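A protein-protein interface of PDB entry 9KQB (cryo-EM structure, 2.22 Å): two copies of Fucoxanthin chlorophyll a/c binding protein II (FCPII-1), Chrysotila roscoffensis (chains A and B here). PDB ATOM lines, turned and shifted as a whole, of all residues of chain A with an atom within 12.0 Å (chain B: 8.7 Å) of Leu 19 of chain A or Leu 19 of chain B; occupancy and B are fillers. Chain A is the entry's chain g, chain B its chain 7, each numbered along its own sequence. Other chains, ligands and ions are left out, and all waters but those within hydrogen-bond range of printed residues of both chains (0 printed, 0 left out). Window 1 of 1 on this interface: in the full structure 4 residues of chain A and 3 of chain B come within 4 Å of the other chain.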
ATOM      1  N   THR A  13      26.880  23.080 -18.568  1.00  0.00           N
ATOM      2  CA  THR A  13      26.678  21.697 -18.973  1.00  0.00           C
ATOM      3  C   THR A  13      27.653  21.270 -20.056  1.00  0.00           C
ATOM      4  O   THR A  13      28.446  20.345 -19.844  1.00  0.00           O
ATOM      5  CB  THR A  13      25.236  21.486 -19.465  1.00  0.00           C
ATOM      6  OG1 THR A  13      25.058  22.146 -20.725  1.00  0.00           O
ATOM      7  CG2 THR A  13      24.232  22.036 -18.462  1.00  0.00           C
ATOM      8  N   GLY A  14      27.617  21.923 -21.213  1.00  0.00           N
ATOM      9  CA  GLY A  14      28.548  21.655 -22.289  1.00  0.00           C
ATOM     10  C   GLY A  14      28.001  20.608 -23.231  1.00  0.00           C
ATOM     11  O   GLY A  14      28.128  19.414 -22.940  1.00  0.00           O
ATOM     12  N   PHE A  15      27.457  21.037 -24.373  1.00  0.00           N
ATOM     13  CA  PHE A  15      26.836  20.157 -25.366  1.00  0.00           C
ATOM     14  C   PHE A  15      25.817  19.224 -24.710  1.00  0.00           C
ATOM     15  O   PHE A  15      26.052  18.024 -24.560  1.00  0.00           O
ATOM     16  CB  PHE A  15      27.883  19.368 -26.153  1.00  0.00           C
ATOM     17  CG  PHE A  15      27.340  18.741 -27.402  1.00  0.00           C
ATOM     18  CD1 PHE A  15      26.779  19.527 -28.395  1.00  0.00           C
ATOM     19  CD2 PHE A  15      27.368  17.368 -27.573  1.00  0.00           C
ATOM     20  CE1 PHE A  15      26.268  18.956 -29.545  1.00  0.00           C
ATOM     21  CE2 PHE A  15      26.858  16.788 -28.719  1.00  0.00           C
ATOM     22  CZ  PHE A  15      26.307  17.584 -29.707  1.00  0.00           C
ATOM     23  N   PHE A  16      24.706  19.829 -24.264  1.00  0.00           N
ATOM     24  CA  PHE A  16      23.742  19.158 -23.391  1.00  0.00           C
ATOM     25  C   PHE A  16      23.224  17.857 -24.000  1.00  0.00           C
ATOM     26  O   PHE A  16      23.580  16.769 -23.531  1.00  0.00           O
ATOM     27  CB  PHE A  16      22.583  20.117 -23.104  1.00  0.00           C
ATOM     28  CG  PHE A  16      21.657  19.656 -22.017  1.00  0.00           C
ATOM     29  CD1 PHE A  16      22.141  18.981 -20.910  1.00  0.00           C
ATOM     30  CD2 PHE A  16      20.299  19.909 -22.104  1.00  0.00           C
ATOM     31  CE1 PHE A  16      21.282  18.561 -19.911  1.00  0.00           C
ATOM     32  CE2 PHE A  16      19.435  19.494 -21.112  1.00  0.00           C
ATOM     33  CZ  PHE A  16      19.927  18.817 -20.013  1.00  0.00           C
ATOM     34  N   ASP A  17      22.429  17.966 -25.072  1.00  0.00           N
ATOM     35  CA  ASP A  17      21.923  16.887 -25.922  1.00  0.00           C
ATOM     36  C   ASP A  17      21.717  15.515 -25.255  1.00  0.00           C
ATOM     37  O   ASP A  17      22.385  14.545 -25.622  1.00  0.00           O
ATOM     38  CB  ASP A  17      22.803  16.749 -27.160  1.00  0.00           C
ATOM     39  CG  ASP A  17      22.084  16.085 -28.316  1.00  0.00           C
ATOM     40  OD1 ASP A  17      20.837  16.151 -28.359  1.00  0.00           O
ATOM     41  OD2 ASP A  17      22.765  15.499 -29.183  1.00  0.00           O
ATOM     42  N   PRO A  18      20.812  15.409 -24.261  1.00  0.00           N
ATOM     43  CA  PRO A  18      20.624  14.109 -23.601  1.00  0.00           C
ATOM     44  C   PRO A  18      19.921  13.096 -24.490  1.00  0.00           C
ATOM     45  O   PRO A  18      20.295  11.919 -24.521  1.00  0.00           O
ATOM     46  CB  PRO A  18      19.773  14.455 -22.369  1.00  0.00           C
ATOM     47  CG  PRO A  18      19.868  15.941 -22.228  1.00  0.00           C
ATOM     48  CD  PRO A  18      19.983  16.444 -23.625  1.00  0.00           C
ATOM     49  N   LEU A  19      18.898  13.549 -25.217  1.00  0.00           N
ATOM     50  CA  LEU A  19      18.146  12.648 -26.083  1.00  0.00           C
ATOM     51  C   LEU A  19      18.963  12.233 -27.300  1.00  0.00           C
ATOM     52  O   LEU A  19      18.831  11.107 -27.792  1.00  0.00           O
ATOM     53  CB  LEU A  19      16.839  13.312 -26.520  1.00  0.00           C
ATOM     54  CG  LEU A  19      15.788  13.577 -25.440  1.00  0.00           C
ATOM     55  CD1 LEU A  19      14.442  13.888 -26.074  1.00  0.00           C
ATOM     56  CD2 LEU A  19      15.670  12.400 -24.482  1.00  0.00           C
ATOM     57  N   GLY A  20      19.812  13.123 -27.796  1.00  0.00           N
ATOM     58  CA  GLY A  20      20.568  12.866 -29.000  1.00  0.00           C
ATOM     59  C   GLY A  20      19.904  13.334 -30.274  1.00  0.00           C
ATOM     60  O   GLY A  20      20.097  12.700 -31.317  1.00  0.00           O
ATOM     61  N   LEU A  21      19.124  14.416 -30.219  1.00  0.00           N
ATOM     62  CA  LEU A  21      18.418  14.899 -31.401  1.00  0.00           C
ATOM     63  C   LEU A  21      19.376  15.488 -32.427  1.00  0.00           C
ATOM     64  O   LEU A  21      19.060  15.523 -33.622  1.00  0.00           O
ATOM     65  CB  LEU A  21      17.367  15.928 -30.986  1.00  0.00           C
ATOM     66  CG  LEU A  21      16.434  15.477 -29.857  1.00  0.00           C
ATOM     67  CD1 LEU A  21      15.378  16.523 -29.569  1.00  0.00           C
ATOM     68  CD2 LEU A  21      15.773  14.147 -30.195  1.00  0.00           C
ATOM     69  N   SER A  22      20.543  15.952 -31.987  1.00  0.00           N
ATOM     70  CA  SER A  22      21.564  16.464 -32.889  1.00  0.00           C
ATOM     71  C   SER A  22      22.491  15.377 -33.412  1.00  0.00           C
ATOM     72  O   SER A  22      23.373  15.675 -34.225  1.00  0.00           O
ATOM     73  CB  SER A  22      22.396  17.542 -32.189  1.00  0.00           C
ATOM     74  OG  SER A  22      23.368  16.958 -31.340  1.00  0.00           O
ATOM     75  N   ALA A  23      22.319  14.136 -32.968  1.00  0.00           N
ATOM     76  CA  ALA A  23      23.190  13.055 -33.409  1.00  0.00           C
ATOM     77  C   ALA A  23      22.734  12.520 -34.761  1.00  0.00           C
ATOM     78  O   ALA A  23      21.553  12.211 -34.949  1.00  0.00           O
ATOM     79  CB  ALA A  23      23.206  11.933 -32.373  1.00  0.00           C
ATOM     80  N   ASN A  24      23.686  12.426 -35.697  1.00  0.00           N
ATOM     81  CA  ASN A  24      23.481  11.858 -37.034  1.00  0.00           C
ATOM     82  C   ASN A  24      22.396  12.601 -37.816  1.00  0.00           C
ATOM     83  O   ASN A  24      21.436  12.009 -38.314  1.00  0.00           O
ATOM     84  CB  ASN A  24      23.178  10.359 -36.957  1.00  0.00           C
ATOM     85  CG  ASN A  24      24.087   9.631 -35.985  1.00  0.00           C
ATOM     86  OD1 ASN A  24      23.664   9.236 -34.899  1.00  0.00           O
ATOM     87  ND2 ASN A  24      25.347   9.457 -36.369  1.00  0.00           N
ATOM     88  N   ILE A  25      22.557  13.918 -37.917  1.00  0.00           N
ATOM     89  CA  ILE A  25      21.727  14.761 -38.769  1.00  0.00           C
ATOM     90  C   ILE A  25      22.661  15.587 -39.642  1.00  0.00           C
ATOM     91  O   ILE A  25      23.793  15.880 -39.243  1.00  0.00           O
ATOM     92  CB  ILE A  25      20.781  15.669 -37.954  1.00  0.00           C
ATOM     93  CG1 ILE A  25      21.560  16.468 -36.908  1.00  0.00           C
ATOM     94  CG2 ILE A  25      19.688  14.845 -37.290  1.00  0.00           C
ATOM     95  CD1 ILE A  25      20.808  17.673 -36.383  1.00  0.00           C
ATOM     96  N   TYR A  33      17.745  23.751 -37.091  1.00  0.00           N
ATOM     97  CA  TYR A  33      17.534  23.755 -35.647  1.00  0.00           C
ATOM     98  C   TYR A  33      18.044  25.048 -35.021  1.00  0.00           C
ATOM     99  O   TYR A  33      17.432  25.582 -34.089  1.00  0.00           O
ATOM    100  CB  TYR A  33      18.243  22.553 -35.018  1.00  0.00           C
ATOM    101  CG  TYR A  33      17.524  21.218 -35.099  1.00  0.00           C
ATOM    102  CD1 TYR A  33      16.558  20.966 -36.066  1.00  0.00           C
ATOM    103  CD2 TYR A  33      17.846  20.195 -34.219  1.00  0.00           C
ATOM    104  CE1 TYR A  33      15.921  19.738 -36.138  1.00  0.00           C
ATOM    105  CE2 TYR A  33      17.213  18.970 -34.280  1.00  0.00           C
ATOM    106  CZ  TYR A  33      16.252  18.744 -35.239  1.00  0.00           C
ATOM    107  OH  TYR A  33      15.627  17.519 -35.294  1.00  0.00           O
ATOM    108  N   PHE B  16      16.381  -3.121 -26.864  1.00  0.00           N
ATOM    109  CA  PHE B  16      15.348  -2.100 -26.716  1.00  0.00           C
ATOM    110  C   PHE B  16      16.020  -0.748 -26.498  1.00  0.00           C
ATOM    111  O   PHE B  16      16.486  -0.443 -25.397  1.00  0.00           O
ATOM    112  CB  PHE B  16      14.408  -2.458 -25.569  1.00  0.00           C
ATOM    113  CG  PHE B  16      13.269  -1.500 -25.397  1.00  0.00           C
ATOM    114  CD1 PHE B  16      12.489  -1.127 -26.478  1.00  0.00           C
ATOM    115  CD2 PHE B  16      12.963  -0.989 -24.150  1.00  0.00           C
ATOM    116  CE1 PHE B  16      11.435  -0.246 -26.318  1.00  0.00           C
ATOM    117  CE2 PHE B  16      11.915  -0.105 -23.982  1.00  0.00           C
ATOM    118  CZ  PHE B  16      11.149   0.266 -25.068  1.00  0.00           C
ATOM    119  N   ASP B  17      16.069   0.057 -27.557  1.00  0.00           N
ATOM    120  CA  ASP B  17      16.611   1.418 -27.503  1.00  0.00           C
ATOM    121  C   ASP B  17      15.858   2.298 -28.492  1.00  0.00           C
ATOM    122  O   ASP B  17      16.387   2.669 -29.546  1.00  0.00           O
ATOM    123  CB  ASP B  17      18.110   1.417 -27.805  1.00  0.00           C
ATOM    124  CG  ASP B  17      18.897   2.277 -26.842  1.00  0.00           C
ATOM    125  OD1 ASP B  17      18.373   2.597 -25.757  1.00  0.00           O
ATOM    126  OD2 ASP B  17      20.042   2.641 -27.181  1.00  0.00           O
ATOM    127  N   PRO B  18      14.610   2.661 -28.179  1.00  0.00           N
ATOM    128  CA  PRO B  18      13.858   3.506 -29.115  1.00  0.00           C
ATOM    129  C   PRO B  18      14.296   4.960 -29.091  1.00  0.00           C
ATOM    130  O   PRO B  18      14.183   5.643 -30.115  1.00  0.00           O
ATOM    131  CB  PRO B  18      12.409   3.340 -28.644  1.00  0.00           C
ATOM    132  CG  PRO B  18      12.534   3.106 -27.183  1.00  0.00           C
ATOM    133  CD  PRO B  18      13.821   2.343 -26.975  1.00  0.00           C
ATOM    134  N   LEU B  19      14.789   5.452 -27.958  1.00  0.00           N
ATOM    135  CA  LEU B  19      15.245   6.830 -27.841  1.00  0.00           C
ATOM    136  C   LEU B  19      16.717   6.999 -28.189  1.00  0.00           C
ATOM    137  O   LEU B  19      17.189   8.137 -28.272  1.00  0.00           O
ATOM    138  CB  LEU B  19      14.988   7.351 -26.423  1.00  0.00           C
ATOM    139  CG  LEU B  19      13.610   7.969 -26.171  1.00  0.00           C
ATOM    140  CD1 LEU B  19      13.559   8.628 -24.803  1.00  0.00           C
ATOM    141  CD2 LEU B  19      13.253   8.966 -27.262  1.00  0.00           C
ATOM    142  N   GLY B  20      17.442   5.904 -28.402  1.00  0.00           N
ATOM    143  CA  GLY B  20      18.845   5.967 -28.763  1.00  0.00           C
ATOM    144  C   GLY B  20      19.739   6.543 -27.686  1.00  0.00           C
ATOM    145  O   GLY B  20      20.610   7.370 -27.973  1.00  0.00           O
ATOM    146  N   LEU B  21      19.539   6.114 -26.441  1.00  0.00           N
ATOM    147  CA  LEU B  21      20.312   6.607 -25.308  1.00  0.00           C
ATOM    148  C   LEU B  21      21.576   5.793 -25.063  1.00  0.00           C
ATOM    149  O   LEU B  21      22.216   5.955 -24.018  1.00  0.00           O
ATOM    150  CB  LEU B  21      19.446   6.634 -24.049  1.00  0.00           C
ATOM    151  CG  LEU B  21      18.198   7.515 -24.122  1.00  0.00           C
ATOM    152  CD1 LEU B  21      17.431   7.473 -22.811  1.00  0.00           C
ATOM    153  CD2 LEU B  21      18.576   8.941 -24.482  1.00  0.00           C
ATOM    154  N   SER B  22      21.945   4.916 -25.995  1.00  0.00           N
ATOM    155  CA  SER B  22      23.151   4.115 -25.862  1.00  0.00           C
ATOM    156  C   SER B  22      23.985   4.046 -27.131  1.00  0.00           C
ATOM    157  O   SER B  22      25.036   3.394 -27.118  1.00  0.00           O
ATOM    158  CB  SER B  22      22.801   2.684 -25.421  1.00  0.00           C
ATOM    159  OG  SER B  22      23.934   2.012 -24.913  1.00  0.00           O
ATOM    160  N   ALA B  23      23.560   4.689 -28.220  1.00  0.00           N
ATOM    161  CA  ALA B  23      24.306   4.616 -29.470  1.00  0.00           C
ATOM    162  C   ALA B  23      25.576   5.458 -29.411  1.00  0.00           C
ATOM    163  O   ALA B  23      26.629   5.046 -29.912  1.00  0.00           O
ATOM    164  CB  ALA B  23      23.420   5.059 -30.635  1.00  0.00           C
ATOM    165  N   ASN B  24      25.498   6.639 -28.802  1.00  0.00           N
ATOM    166  CA  ASN B  24      26.618   7.568 -28.752  1.00  0.00           C
ATOM    167  C   ASN B  24      27.269   7.649 -27.376  1.00  0.00           C
ATOM    168  O   ASN B  24      27.937   8.645 -27.079  1.00  0.00           O
ATOM    169  CB  ASN B  24      26.166   8.961 -29.195  1.00  0.00           C
ATOM    170  CG  ASN B  24      25.099   8.915 -30.270  1.00  0.00           C
ATOM    171  OD1 ASN B  24      23.912   9.079 -29.989  1.00  0.00           O
ATOM    172  ND2 ASN B  24      25.518   8.693 -31.510  1.00  0.00           N
ATOM    173  N   ILE B  25      27.094   6.634 -26.532  1.00  0.00           N
ATOM    174  CA  ILE B  25      27.701   6.637 -25.204  1.00  0.00           C
ATOM    175  C   ILE B  25      28.935   5.745 -25.208  1.00  0.00           C
ATOM    176  O   ILE B  25      29.133   4.942 -26.126  1.00  0.00           O
ATOM    177  CB  ILE B  25      26.692   6.192 -24.130  1.00  0.00           C
ATOM    178  CG1 ILE B  25      26.458   4.682 -24.208  1.00  0.00           C
ATOM    179  CG2 ILE B  25      25.382   6.951 -24.280  1.00  0.00           C
ATOM    180  CD1 ILE B  25      25.976   4.076 -22.914  1.00  0.00           C
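Of the printed residues of chain B, Pro 18 of chain A touches Leu 21 (3.4 Å). Leu 19 of chain A touches just these residues of chain B: Leu 19 and Leu 21. Printed residues of chain B within 4 Å of Ala 23 of chain A: Asn 24 (3.8 Å). Of the printed residues of chain B, Asn 24 of chain A touches Asn 24. No residue of chain A comes within 4 Å of Asp 17 of chain B. Leu 19 of chain B touches just one residue of chain A: Leu 19 (3.4 Å). No residue of chain A comes within 4 Å of Gly 20 of chain B. Of the printed residues of chain A, Asn 24 of chain B touches Ala 23 and Asn 24. The nearest residue of chain B that does not touch Leu 19 of chain A is Gly 20 of chain B (4.1 Å).
Of the 10 printed residues of chain B, 3 touch a printed residue of chain A. Of the 14 printed residues of chain A, 4 touch a printed residue of chain B. Hydrophobic or aromatic side chains of chain A within 4 Å of the printed part of chain B: Ala 23. Among the printed residues, 5 pairs touch across the chains.
Among the printed residues, pairs that only touch across the chains: Pro 18 of chain A with Leu 21 of chain B, Ala 23 of chain A with Asn 24 of chain B, Asn 24 of chain A with Asn 24 of chain B and Leu 19 of chain A with Leu 21 of chain B.
Pro 18 of chain A touches Leu 21 of chain B, but with the chains exchanged Leu 21 of chain A does not touch Pro 18 of chain B (8.7 Å). Leu 19 of chain A touches its own counterpart, Leu 19 of chain B. Ala 23 of chain A touches Asn 24 of chain B, but with the chains exchanged Asn 24 of chain A does not touch Ala 23 of chain B (6.0 Å). Asn 24 of chain A touches its own counterpart, Asn 24 of chain B. Of the 5 pairs that touch across the chains among the printed residues, 2 have their exchanged pair printed and touching as well.
O of Leu 19 of chain A lies close to O of Leu 19 of chain B, at 3.4 Å.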
